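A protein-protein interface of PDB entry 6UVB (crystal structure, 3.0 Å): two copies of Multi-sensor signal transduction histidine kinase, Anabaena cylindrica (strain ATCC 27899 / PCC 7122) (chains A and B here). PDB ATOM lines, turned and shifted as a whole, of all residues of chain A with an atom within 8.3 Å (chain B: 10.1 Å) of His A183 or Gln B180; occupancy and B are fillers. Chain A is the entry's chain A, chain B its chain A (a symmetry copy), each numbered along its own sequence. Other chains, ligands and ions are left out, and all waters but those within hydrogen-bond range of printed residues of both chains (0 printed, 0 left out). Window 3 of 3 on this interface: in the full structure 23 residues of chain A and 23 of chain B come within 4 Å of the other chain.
The backbone NH of His B183 lies within hydrogen-bond range of the side-chain amide oxygen of Gln A180, at 3.4 Å.
The side-chain amide oxygen of Gln B180 sits at hydrogen-bond distance from the backbone NH of His A183, 3.4 Å away.
The backbone carbonyl oxygen (O) of Gln B180 lies close to the backbone carbonyl oxygen (O) of Gln A180 (3.2 Å).
The backbone carbonyl oxygen of Ile A17 is in hydrogen-bond range of the side-chain hydroxyl of Thr A20.
Gln B173 touches Ile A17 (O to CD1, 3.7 Å).
Ile A17 touches Leu B174.
Thr A20 touches Thr B20 (CG2 to CG2, 3.6 Å).
Leu A21 touches Ala B177 (CD2 to CA, 3.5 Å).
Gln B180 touches Leu A21.
Leu B181 touches Leu A21 (CD1 to CD1, 3.6 Å).
Ala A177 touches Leu B21 (CA to CD2, 3.5 Å).
Gln A180 touches Leu B21 (CB to CD1, 3.6 Å).
CD1 of Leu A181 touches CD1 of Leu B21, 3.6 Å away.
Of the printed residues of chain B, Leu A181 touches Leu B21 (3.6 Å).
Of chain B, only Gln B180 comes within 4 Å of His A183.
Of the printed residues of chain A, Thr B20 touches Thr A20.
Glu B126 touches none of the printed residues of chain A.
Of the printed residues of chain A, Gln B173 touches Ile A17 (3.7 Å).
Of the printed residues of chain A, Leu B181 touches Leu A21 (3.6 Å).
The nearest printed residue of chain A that does not touch Gln B180 is Leu A181 (4.01 Å).
The nearest printed residue of chain A that does not touch Leu B174 is Leu A21 (7.0 Å).
Of the 21 printed residues of chain B, 8 touch a printed residue of chain A.
Hydrophobic or aromatic side chains of chain B that line the printed part of chain A: Leu B21, Leu B174, Ala B177, Leu B181 and His B183.
Of the 12 printed residues of chain A, 7 touch a printed residue of chain B.
Hydrophobic or aromatic side chains of chain A that line the printed part of chain B: Ile A17, Leu A21, Ala A177, Leu A181 and His A183.
Among the printed residues, 12 pairs touch across the chains.
Among the printed residues, no Asp or Glu carboxylate lies within 4 Å of a Lys or Arg side-chain nitrogen of the other chain.
Thr B20 touches its own counterpart, Thr A20.
Leu A21 touches Ala B177, and with the chains exchanged Ala A177 touches Leu B21.
Leu A21 touches Gln B180, and with the chains exchanged Gln A180 touches Leu B21.
Leu A21 touches Leu B181, and with the chains exchanged Leu A181 touches Leu B21.
Positions printed for both chains: 20, 21, 22, 23, 177, 178, 179, 180, 181, 182 and 183.
Of the 12 pairs that touch across the chains among the printed residues, 10 have their exchanged pair printed and touching as well.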
ATOM      1  N   ILE A  17      19.306 -19.088   9.903  1.00  0.00           N
ATOM      2  CA  ILE A  17      19.514 -17.747   9.370  1.00  0.00           C
ATOM      3  C   ILE A  17      20.692 -17.732   8.399  1.00  0.00           C
ATOM      4  O   ILE A  17      20.538 -17.368   7.229  1.00  0.00           O
ATOM      5  CB  ILE A  17      19.693 -16.744  10.522  1.00  0.00           C
ATOM      6  CG1 ILE A  17      18.381 -16.628  11.290  1.00  0.00           C
ATOM      7  CG2 ILE A  17      20.139 -15.387  10.013  1.00  0.00           C
ATOM      8  CD1 ILE A  17      18.275 -15.404  12.138  1.00  0.00           C
ATOM      9  N   THR A  20      19.701 -20.012   5.186  1.00  0.00           N
ATOM     10  CA  THR A  20      18.815 -19.426   4.185  1.00  0.00           C
ATOM     11  C   THR A  20      19.390 -18.161   3.548  1.00  0.00           C
ATOM     12  O   THR A  20      19.044 -17.852   2.400  1.00  0.00           O
ATOM     13  CB  THR A  20      17.440 -19.144   4.827  1.00  0.00           C
ATOM     14  OG1 THR A  20      17.596 -18.572   6.140  1.00  0.00           O
ATOM     15  CG2 THR A  20      16.639 -20.437   4.964  1.00  0.00           C
ATOM     16  N   LEU A  21      20.299 -17.459   4.240  1.00  0.00           N
ATOM     17  CA  LEU A  21      20.721 -16.112   3.849  1.00  0.00           C
ATOM     18  C   LEU A  21      22.022 -16.054   3.053  1.00  0.00           C
ATOM     19  O   LEU A  21      22.264 -15.056   2.357  1.00  0.00           O
ATOM     20  CB  LEU A  21      20.869 -15.218   5.090  1.00  0.00           C
ATOM     21  CG  LEU A  21      21.231 -13.743   4.848  1.00  0.00           C
ATOM     22  CD1 LEU A  21      20.246 -13.116   3.857  1.00  0.00           C
ATOM     23  CD2 LEU A  21      21.316 -12.942   6.146  1.00  0.00           C
ATOM     24  N   ASN A  22      22.862 -17.076   3.131  1.00  0.00           N
ATOM     25  CA  ASN A  22      24.021 -17.138   2.254  1.00  0.00           C
ATOM     26  C   ASN A  22      23.608 -17.727   0.909  1.00  0.00           C
ATOM     27  O   ASN A  22      22.789 -18.650   0.848  1.00  0.00           O
ATOM     28  CB  ASN A  22      25.132 -17.949   2.926  1.00  0.00           C
ATOM     29  CG  ASN A  22      25.646 -19.082   2.072  1.00  0.00           C
ATOM     30  OD1 ASN A  22      24.990 -20.115   1.927  1.00  0.00           O
ATOM     31  ND2 ASN A  22      26.851 -18.917   1.545  1.00  0.00           N
ATOM     32  N   VAL A  23      24.150 -17.156  -0.176  1.00  0.00           N
ATOM     33  CA  VAL A  23      23.680 -17.500  -1.524  1.00  0.00           C
ATOM     34  C   VAL A  23      24.003 -18.957  -1.867  1.00  0.00           C
ATOM     35  O   VAL A  23      23.145 -19.686  -2.386  1.00  0.00           O
ATOM     36  CB  VAL A  23      24.266 -16.543  -2.587  1.00  0.00           C
ATOM     37  CG1 VAL A  23      23.239 -16.255  -3.665  1.00  0.00           C
ATOM     38  CG2 VAL A  23      24.758 -15.249  -1.961  1.00  0.00           C
ATOM     39  N   ALA A 177      16.829 -13.856  -6.920  1.00  0.00           N
ATOM     40  CA  ALA A 177      17.343 -14.227  -5.608  1.00  0.00           C
ATOM     41  C   ALA A 177      18.785 -13.769  -5.420  1.00  0.00           C
ATOM     42  O   ALA A 177      19.199 -13.454  -4.293  1.00  0.00           O
ATOM     43  CB  ALA A 177      17.211 -15.740  -5.421  1.00  0.00           C
ATOM     44  N   ILE A 178      19.554 -13.696  -6.506  1.00  0.00           N
ATOM     45  CA  ILE A 178      20.948 -13.285  -6.396  1.00  0.00           C
ATOM     46  C   ILE A 178      21.057 -11.773  -6.224  1.00  0.00           C
ATOM     47  O   ILE A 178      21.845 -11.292  -5.398  1.00  0.00           O
ATOM     48  CB  ILE A 178      21.738 -13.800  -7.615  1.00  0.00           C
ATOM     49  CG1 ILE A 178      22.271 -15.208  -7.322  1.00  0.00           C
ATOM     50  CG2 ILE A 178      22.874 -12.855  -7.979  1.00  0.00           C
ATOM     51  CD1 ILE A 178      22.503 -16.044  -8.552  1.00  0.00           C
ATOM     52  N   GLN A 179      20.259 -11.005  -6.982  1.00  0.00           N
ATOM     53  CA  GLN A 179      20.204  -9.551  -6.826  1.00  0.00           C
ATOM     54  C   GLN A 179      19.992  -9.137  -5.370  1.00  0.00           C
ATOM     55  O   GLN A 179      20.337  -8.009  -4.985  1.00  0.00           O
ATOM     56  CB  GLN A 179      19.080  -8.983  -7.712  1.00  0.00           C
ATOM     57  CG  GLN A 179      19.054  -7.447  -7.835  1.00  0.00           C
ATOM     58  CD  GLN A 179      18.272  -6.932  -9.056  1.00  0.00           C
ATOM     59  OE1 GLN A 179      18.142  -7.623 -10.079  1.00  0.00           O
ATOM     60  NE2 GLN A 179      17.766  -5.701  -8.951  1.00  0.00           N
ATOM     61  N   GLN A 180      19.461 -10.041  -4.549  1.00  0.00           N
ATOM     62  CA  GLN A 180      19.127  -9.777  -3.161  1.00  0.00           C
ATOM     63  C   GLN A 180      20.281 -10.040  -2.189  1.00  0.00           C
ATOM     64  O   GLN A 180      20.432  -9.301  -1.209  1.00  0.00           O
ATOM     65  CB  GLN A 180      17.916 -10.624  -2.765  1.00  0.00           C
ATOM     66  CG  GLN A 180      16.562 -10.021  -3.142  1.00  0.00           C
ATOM     67  CD  GLN A 180      16.015  -9.094  -2.057  1.00  0.00           C
ATOM     68  OE1 GLN A 180      16.517  -7.989  -1.869  1.00  0.00           O
ATOM     69  NE2 GLN A 180      14.985  -9.546  -1.340  1.00  0.00           N
ATOM     70  N   LEU A 181      21.103 -11.068  -2.422  1.00  0.00           N
ATOM     71  CA  LEU A 181      22.044 -11.571  -1.410  1.00  0.00           C
ATOM     72  C   LEU A 181      23.509 -11.196  -1.681  1.00  0.00           C
ATOM     73  O   LEU A 181      24.409 -12.004  -1.412  1.00  0.00           O
ATOM     74  CB  LEU A 181      21.910 -13.091  -1.280  1.00  0.00           C
ATOM     75  CG  LEU A 181      20.875 -13.762  -0.370  1.00  0.00           C
ATOM     76  CD1 LEU A 181      19.487 -13.199  -0.594  1.00  0.00           C
ATOM     77  CD2 LEU A 181      20.877 -15.273  -0.593  1.00  0.00           C
ATOM     78  N   GLU A 182      23.804  -9.978  -2.155  1.00  0.00           N
ATOM     79  CA  GLU A 182      25.166  -9.605  -2.541  1.00  0.00           C
ATOM     80  C   GLU A 182      25.869  -8.641  -1.577  1.00  0.00           C
ATOM     81  O   GLU A 182      26.992  -8.213  -1.873  1.00  0.00           O
ATOM     82  CB  GLU A 182      25.171  -8.982  -3.948  1.00  0.00           C
ATOM     83  CG  GLU A 182      24.752  -9.907  -5.102  1.00  0.00           C
ATOM     84  CD  GLU A 182      25.844 -10.885  -5.546  1.00  0.00           C
ATOM     85  OE1 GLU A 182      26.279 -11.695  -4.699  1.00  0.00           O
ATOM     86  OE2 GLU A 182      26.256 -10.851  -6.735  1.00  0.00           O
ATOM     87  N   HIS A 183      25.243  -8.272  -0.454  1.00  0.00           N
ATOM     88  CA  HIS A 183      25.845  -7.381   0.562  1.00  0.00           C
ATOM     89  C   HIS A 183      26.137  -5.965   0.055  1.00  0.00           C
ATOM     90  O   HIS A 183      26.178  -5.006   0.839  1.00  0.00           O
ATOM     91  CB  HIS A 183      27.139  -7.993   1.125  1.00  0.00           C
ATOM     92  CG  HIS A 183      26.980  -9.398   1.619  1.00  0.00           C
ATOM     93  ND1 HIS A 183      26.974 -10.490   0.774  1.00  0.00           N
ATOM     94  CD2 HIS A 183      26.821  -9.894   2.869  1.00  0.00           C
ATOM     95  CE1 HIS A 183      26.821 -11.593   1.479  1.00  0.00           C
ATOM     96  NE2 HIS A 183      26.723 -11.261   2.756  1.00  0.00           N
ATOM     97  N   THR B  20      12.102 -18.507   1.217  1.00  0.00           N
ATOM     98  CA  THR B  20      13.321 -18.152   1.936  1.00  0.00           C
ATOM     99  C   THR B  20      13.715 -16.686   1.756  1.00  0.00           C
ATOM    100  O   THR B  20      14.369 -16.123   2.643  1.00  0.00           O
ATOM    101  CB  THR B  20      14.465 -19.089   1.490  1.00  0.00           C
ATOM    102  OG1 THR B  20      14.445 -19.274   0.061  1.00  0.00           O
ATOM    103  CG2 THR B  20      14.322 -20.458   2.150  1.00  0.00           C
ATOM    104  N   LEU B  21      13.282 -16.042   0.662  1.00  0.00           N
ATOM    105  CA  LEU B  21      13.801 -14.734   0.259  1.00  0.00           C
ATOM    106  C   LEU B  21      12.942 -13.546   0.682  1.00  0.00           C
ATOM    107  O   LEU B  21      13.453 -12.417   0.742  1.00  0.00           O
ATOM    108  CB  LEU B  21      13.987 -14.681  -1.266  1.00  0.00           C
ATOM    109  CG  LEU B  21      14.604 -13.397  -1.849  1.00  0.00           C
ATOM    110  CD1 LEU B  21      15.922 -13.079  -1.141  1.00  0.00           C
ATOM    111  CD2 LEU B  21      14.776 -13.470  -3.365  1.00  0.00           C
ATOM    112  N   ASN B  22      11.665 -13.754   0.972  1.00  0.00           N
ATOM    113  CA  ASN B  22      10.861 -12.687   1.548  1.00  0.00           C
ATOM    114  C   ASN B  22      11.080 -12.646   3.057  1.00  0.00           C
ATOM    115  O   ASN B  22      11.203 -13.690   3.706  1.00  0.00           O
ATOM    116  CB  ASN B  22       9.390 -12.894   1.180  1.00  0.00           C
ATOM    117  CG  ASN B  22       8.472 -12.906   2.376  1.00  0.00           C
ATOM    118  OD1 ASN B  22       8.415 -13.884   3.123  1.00  0.00           O
ATOM    119  ND2 ASN B  22       7.704 -11.836   2.535  1.00  0.00           N
ATOM    120  N   VAL B  23      11.173 -11.427   3.607  1.00  0.00           N
ATOM    121  CA  VAL B  23      11.581 -11.259   5.007  1.00  0.00           C
ATOM    122  C   VAL B  23      10.535 -11.844   5.961  1.00  0.00           C
ATOM    123  O   VAL B  23      10.880 -12.559   6.911  1.00  0.00           O
ATOM    124  CB  VAL B  23      11.859  -9.776   5.340  1.00  0.00           C
ATOM    125  CG1 VAL B  23      13.031  -9.658   6.298  1.00  0.00           C
ATOM    126  CG2 VAL B  23      12.114  -8.962   4.084  1.00  0.00           C
ATOM    127  N   ILE B  26      10.687 -15.343   7.306  1.00  0.00           N
ATOM    128  CA  ILE B  26      11.709 -15.682   8.286  1.00  0.00           C
ATOM    129  C   ILE B  26      11.499 -14.937   9.605  1.00  0.00           C
ATOM    130  O   ILE B  26      11.972 -15.404  10.650  1.00  0.00           O
ATOM    131  CB  ILE B  26      13.132 -15.479   7.726  1.00  0.00           C
ATOM    132  CG1 ILE B  26      13.565 -14.020   7.838  1.00  0.00           C
ATOM    133  CG2 ILE B  26      13.248 -16.045   6.266  1.00  0.00           C
ATOM    134  CD1 ILE B  26      14.904 -13.737   7.194  1.00  0.00           C
ATOM    135  N   LEU B 124      19.097  -3.658  15.334  1.00  0.00           N
ATOM    136  CA  LEU B 124      19.932  -2.543  14.886  1.00  0.00           C
ATOM    137  C   LEU B 124      20.519  -2.774  13.499  1.00  0.00           C
ATOM    138  O   LEU B 124      21.166  -3.798  13.247  1.00  0.00           O
ATOM    139  CB  LEU B 124      21.073  -2.291  15.867  1.00  0.00           C
ATOM    140  CG  LEU B 124      20.597  -1.620  17.141  1.00  0.00           C
ATOM    141  CD1 LEU B 124      21.739  -1.552  18.130  1.00  0.00           C
ATOM    142  CD2 LEU B 124      20.082  -0.250  16.769  1.00  0.00           C
ATOM    143  N   GLN B 125      20.335  -1.790  12.623  1.00  0.00           N
ATOM    144  CA  GLN B 125      20.943  -1.771  11.300  1.00  0.00           C
ATOM    145  C   GLN B 125      22.208  -0.927  11.364  1.00  0.00           C
ATOM    146  O   GLN B 125      22.149   0.281  11.628  1.00  0.00           O
ATOM    147  CB  GLN B 125      19.964  -1.234  10.255  1.00  0.00           C
ATOM    148  CG  GLN B 125      18.780  -2.163  10.069  1.00  0.00           C
ATOM    149  CD  GLN B 125      19.224  -3.606   9.829  1.00  0.00           C
ATOM    150  OE1 GLN B 125      20.295  -3.847   9.275  1.00  0.00           O
ATOM    151  NE2 GLN B 125      18.409  -4.569  10.253  1.00  0.00           N
ATOM    152  N   GLU B 126      23.354  -1.564  11.148  1.00  0.00           N
ATOM    153  CA  GLU B 126      24.513  -0.767  10.801  1.00  0.00           C
ATOM    154  C   GLU B 126      24.165  -0.134   9.466  1.00  0.00           C
ATOM    155  O   GLU B 126      24.242  -0.788   8.421  1.00  0.00           O
ATOM    156  CB  GLU B 126      25.792  -1.604  10.738  1.00  0.00           C
ATOM    157  CG  GLU B 126      27.062  -0.769  10.845  1.00  0.00           C
ATOM    158  CD  GLU B 126      28.081  -1.111   9.768  1.00  0.00           C
ATOM    159  OE1 GLU B 126      27.794  -1.999   8.932  1.00  0.00           O
ATOM    160  OE2 GLU B 126      29.167  -0.490   9.753  1.00  0.00           O
ATOM    161  N   GLU B 129      26.631   5.864   5.616  1.00  0.00           N
ATOM    162  CA  GLU B 129      26.363   6.723   4.464  1.00  0.00           C
ATOM    163  C   GLU B 129      25.335   7.802   4.814  1.00  0.00           C
ATOM    164  O   GLU B 129      25.463   8.447   5.862  1.00  0.00           O
ATOM    165  CB  GLU B 129      25.947   5.854   3.270  1.00  0.00           C
ATOM    166  CG  GLU B 129      27.082   4.909   2.862  1.00  0.00           C
ATOM    167  CD  GLU B 129      26.651   3.751   1.994  1.00  0.00           C
ATOM    168  OE1 GLU B 129      25.497   3.298   2.117  1.00  0.00           O
ATOM    169  OE2 GLU B 129      27.481   3.279   1.189  1.00  0.00           O
ATOM    170  N   TRP B 145      16.006  -0.193  13.617  1.00  0.00           N
ATOM    171  CA  TRP B 145      14.965  -0.665  12.711  1.00  0.00           C
ATOM    172  C   TRP B 145      13.654  -0.911  13.457  1.00  0.00           C
ATOM    173  O   TRP B 145      12.576  -0.527  12.985  1.00  0.00           O
ATOM    174  CB  TRP B 145      15.454  -1.933  12.001  1.00  0.00           C
ATOM    175  CG  TRP B 145      14.511  -2.466  10.992  1.00  0.00           C
ATOM    176  CD1 TRP B 145      14.454  -2.148   9.663  1.00  0.00           C
ATOM    177  CD2 TRP B 145      13.474  -3.421  11.224  1.00  0.00           C
ATOM    178  NE1 TRP B 145      13.431  -2.847   9.053  1.00  0.00           N
ATOM    179  CE2 TRP B 145      12.820  -3.639   9.994  1.00  0.00           C
ATOM    180  CE3 TRP B 145      13.033  -4.116  12.353  1.00  0.00           C
ATOM    181  CZ2 TRP B 145      11.748  -4.527   9.868  1.00  0.00           C
ATOM    182  CZ3 TRP B 145      11.964  -5.002  12.218  1.00  0.00           C
ATOM    183  CH2 TRP B 145      11.337  -5.196  10.990  1.00  0.00           C
ATOM    184  N   GLN B 173      20.859 -11.317  15.277  1.00  0.00           N
ATOM    185  CA  GLN B 173      20.880 -12.149  14.076  1.00  0.00           C
ATOM    186  C   GLN B 173      19.792 -11.787  13.069  1.00  0.00           C
ATOM    187  O   GLN B 173      19.903 -12.133  11.882  1.00  0.00           O
ATOM    188  CB  GLN B 173      20.714 -13.610  14.482  1.00  0.00           C
ATOM    189  CG  GLN B 173      21.737 -14.571  13.897  1.00  0.00           C
ATOM    190  CD  GLN B 173      23.165 -14.231  14.275  1.00  0.00           C
ATOM    191  OE1 GLN B 173      23.413 -13.445  15.201  1.00  0.00           O
ATOM    192  NE2 GLN B 173      24.119 -14.830  13.566  1.00  0.00           N
ATOM    193  N   LEU B 174      18.707 -11.160  13.531  1.00  0.00           N
ATOM    194  CA  LEU B 174      17.737 -10.567  12.617  1.00  0.00           C
ATOM    195  C   LEU B 174      18.250  -9.260  12.022  1.00  0.00           C
ATOM    196  O   LEU B 174      17.970  -8.967  10.850  1.00  0.00           O
ATOM    197  CB  LEU B 174      16.422 -10.290  13.336  1.00  0.00           C
ATOM    198  CG  LEU B 174      15.512 -11.449  13.684  1.00  0.00           C
ATOM    199  CD1 LEU B 174      14.094 -10.912  13.827  1.00  0.00           C
ATOM    200  CD2 LEU B 174      15.625 -12.519  12.621  1.00  0.00           C
ATOM    201  N   ALA B 175      18.960  -8.451  12.825  1.00  0.00           N
ATOM    202  CA  ALA B 175      19.594  -7.233  12.327  1.00  0.00           C
ATOM    203  C   ALA B 175      20.355  -7.496  11.032  1.00  0.00           C
ATOM    204  O   ALA B 175      20.192  -6.769  10.046  1.00  0.00           O
ATOM    205  CB  ALA B 175      20.527  -6.673  13.398  1.00  0.00           C
ATOM    206  N   ILE B 176      21.165  -8.560  11.005  1.00  0.00           N
ATOM    207  CA  ILE B 176      21.944  -8.903   9.814  1.00  0.00           C
ATOM    208  C   ILE B 176      21.036  -9.369   8.682  1.00  0.00           C
ATOM    209  O   ILE B 176      21.223  -9.001   7.514  1.00  0.00           O
ATOM    210  CB  ILE B 176      22.968  -9.998  10.145  1.00  0.00           C
ATOM    211  CG1 ILE B 176      24.048  -9.467  11.083  1.00  0.00           C
ATOM    212  CG2 ILE B 176      23.540 -10.580   8.854  1.00  0.00           C
ATOM    213  CD1 ILE B 176      24.384 -10.423  12.208  1.00  0.00           C
ATOM    214  N   ALA B 177      20.083 -10.244   9.009  1.00  0.00           N
ATOM    215  CA  ALA B 177      19.229 -10.830   7.984  1.00  0.00           C
ATOM    216  C   ALA B 177      18.320  -9.785   7.346  1.00  0.00           C
ATOM    217  O   ALA B 177      17.979  -9.895   6.158  1.00  0.00           O
ATOM    218  CB  ALA B 177      18.419 -11.976   8.592  1.00  0.00           C
ATOM    219  N   ILE B 178      17.942  -8.756   8.103  1.00  0.00           N
ATOM    220  CA  ILE B 178      17.057  -7.731   7.563  1.00  0.00           C
ATOM    221  C   ILE B 178      17.821  -6.775   6.653  1.00  0.00           C
ATOM    222  O   ILE B 178      17.334  -6.412   5.574  1.00  0.00           O
ATOM    223  CB  ILE B 178      16.342  -7.003   8.719  1.00  0.00           C
ATOM    224  CG1 ILE B 178      15.047  -7.746   9.069  1.00  0.00           C
ATOM    225  CG2 ILE B 178      16.055  -5.550   8.366  1.00  0.00           C
ATOM    226  CD1 ILE B 178      14.590  -7.545  10.489  1.00  0.00           C
ATOM    227  N   GLN B 179      19.035  -6.371   7.061  1.00  0.00           N
ATOM    228  CA  GLN B 179      19.899  -5.540   6.221  1.00  0.00           C
ATOM    229  C   GLN B 179      20.056  -6.114   4.813  1.00  0.00           C
ATOM    230  O   GLN B 179      20.371  -5.373   3.869  1.00  0.00           O
ATOM    231  CB  GLN B 179      21.277  -5.393   6.894  1.00  0.00           C
ATOM    232  CG  GLN B 179      22.216  -4.355   6.247  1.00  0.00           C
ATOM    233  CD  GLN B 179      23.349  -3.878   7.171  1.00  0.00           C
ATOM    234  OE1 GLN B 179      23.227  -3.896   8.406  1.00  0.00           O
ATOM    235  NE2 GLN B 179      24.450  -3.429   6.564  1.00  0.00           N
ATOM    236  N   GLN B 180      19.805  -7.412   4.650  1.00  0.00           N
ATOM    237  CA  GLN B 180      19.983  -8.120   3.395  1.00  0.00           C
ATOM    238  C   GLN B 180      18.744  -8.094   2.495  1.00  0.00           C
ATOM    239  O   GLN B 180      18.885  -8.012   1.269  1.00  0.00           O
ATOM    240  CB  GLN B 180      20.380  -9.567   3.685  1.00  0.00           C
ATOM    241  CG  GLN B 180      21.872  -9.783   3.946  1.00  0.00           C
ATOM    242  CD  GLN B 180      22.658 -10.037   2.661  1.00  0.00           C
ATOM    243  OE1 GLN B 180      22.870  -9.123   1.868  1.00  0.00           O
ATOM    244  NE2 GLN B 180      23.085 -11.282   2.451  1.00  0.00           N
ATOM    245  N   LEU B 181      17.533  -8.164   3.056  1.00  0.00           N
ATOM    246  CA  LEU B 181      16.316  -8.439   2.277  1.00  0.00           C
ATOM    247  C   LEU B 181      15.421  -7.209   2.067  1.00  0.00           C
ATOM    248  O   LEU B 181      14.188  -7.339   2.079  1.00  0.00           O
ATOM    249  CB  LEU B 181      15.513  -9.563   2.937  1.00  0.00           C
ATOM    250  CG  LEU B 181      15.785 -11.049   2.672  1.00  0.00           C
ATOM    251  CD1 LEU B 181      17.253 -11.384   2.828  1.00  0.00           C
ATOM    252  CD2 LEU B 181      14.941 -11.913   3.606  1.00  0.00           C
ATOM    253  N   GLU B 182      15.979  -6.017   1.820  1.00  0.00           N
ATOM    254  CA  GLU B 182      15.184  -4.791   1.729  1.00  0.00           C
ATOM    255  C   GLU B 182      15.021  -4.233   0.309  1.00  0.00           C
ATOM    256  O   GLU B 182      14.431  -3.155   0.155  1.00  0.00           O
ATOM    257  CB  GLU B 182      15.789  -3.693   2.621  1.00  0.00           C
ATOM    258  CG  GLU B 182      15.783  -3.967   4.134  1.00  0.00           C
ATOM    259  CD  GLU B 182      14.424  -3.743   4.803  1.00  0.00           C
ATOM    260  OE1 GLU B 182      13.458  -4.429   4.403  1.00  0.00           O
ATOM    261  OE2 GLU B 182      14.324  -2.895   5.728  1.00  0.00           O
ATOM    262  N   HIS B 183      15.535  -4.912  -0.721  1.00  0.00           N
ATOM    263  CA  HIS B 183      15.400  -4.486  -2.132  1.00  0.00           C
ATOM    264  C   HIS B 183      16.084  -3.151  -2.446  1.00  0.00           C
ATOM    265  O   HIS B 183      16.474  -2.894  -3.595  1.00  0.00           O
ATOM    266  CB  HIS B 183      13.919  -4.404  -2.535  1.00  0.00           C
ATOM    267  CG  HIS B 183      13.140  -5.647  -2.237  1.00  0.00           C
ATOM    268  ND1 HIS B 183      12.655  -5.941  -0.978  1.00  0.00           N
ATOM    269  CD2 HIS B 183      12.758  -6.676  -3.032  1.00  0.00           C
ATOM    270  CE1 HIS B 183      12.011  -7.090  -1.010  1.00  0.00           C
ATOM    271  NE2 HIS B 183      12.059  -7.560  -2.245  1.00  0.00           N
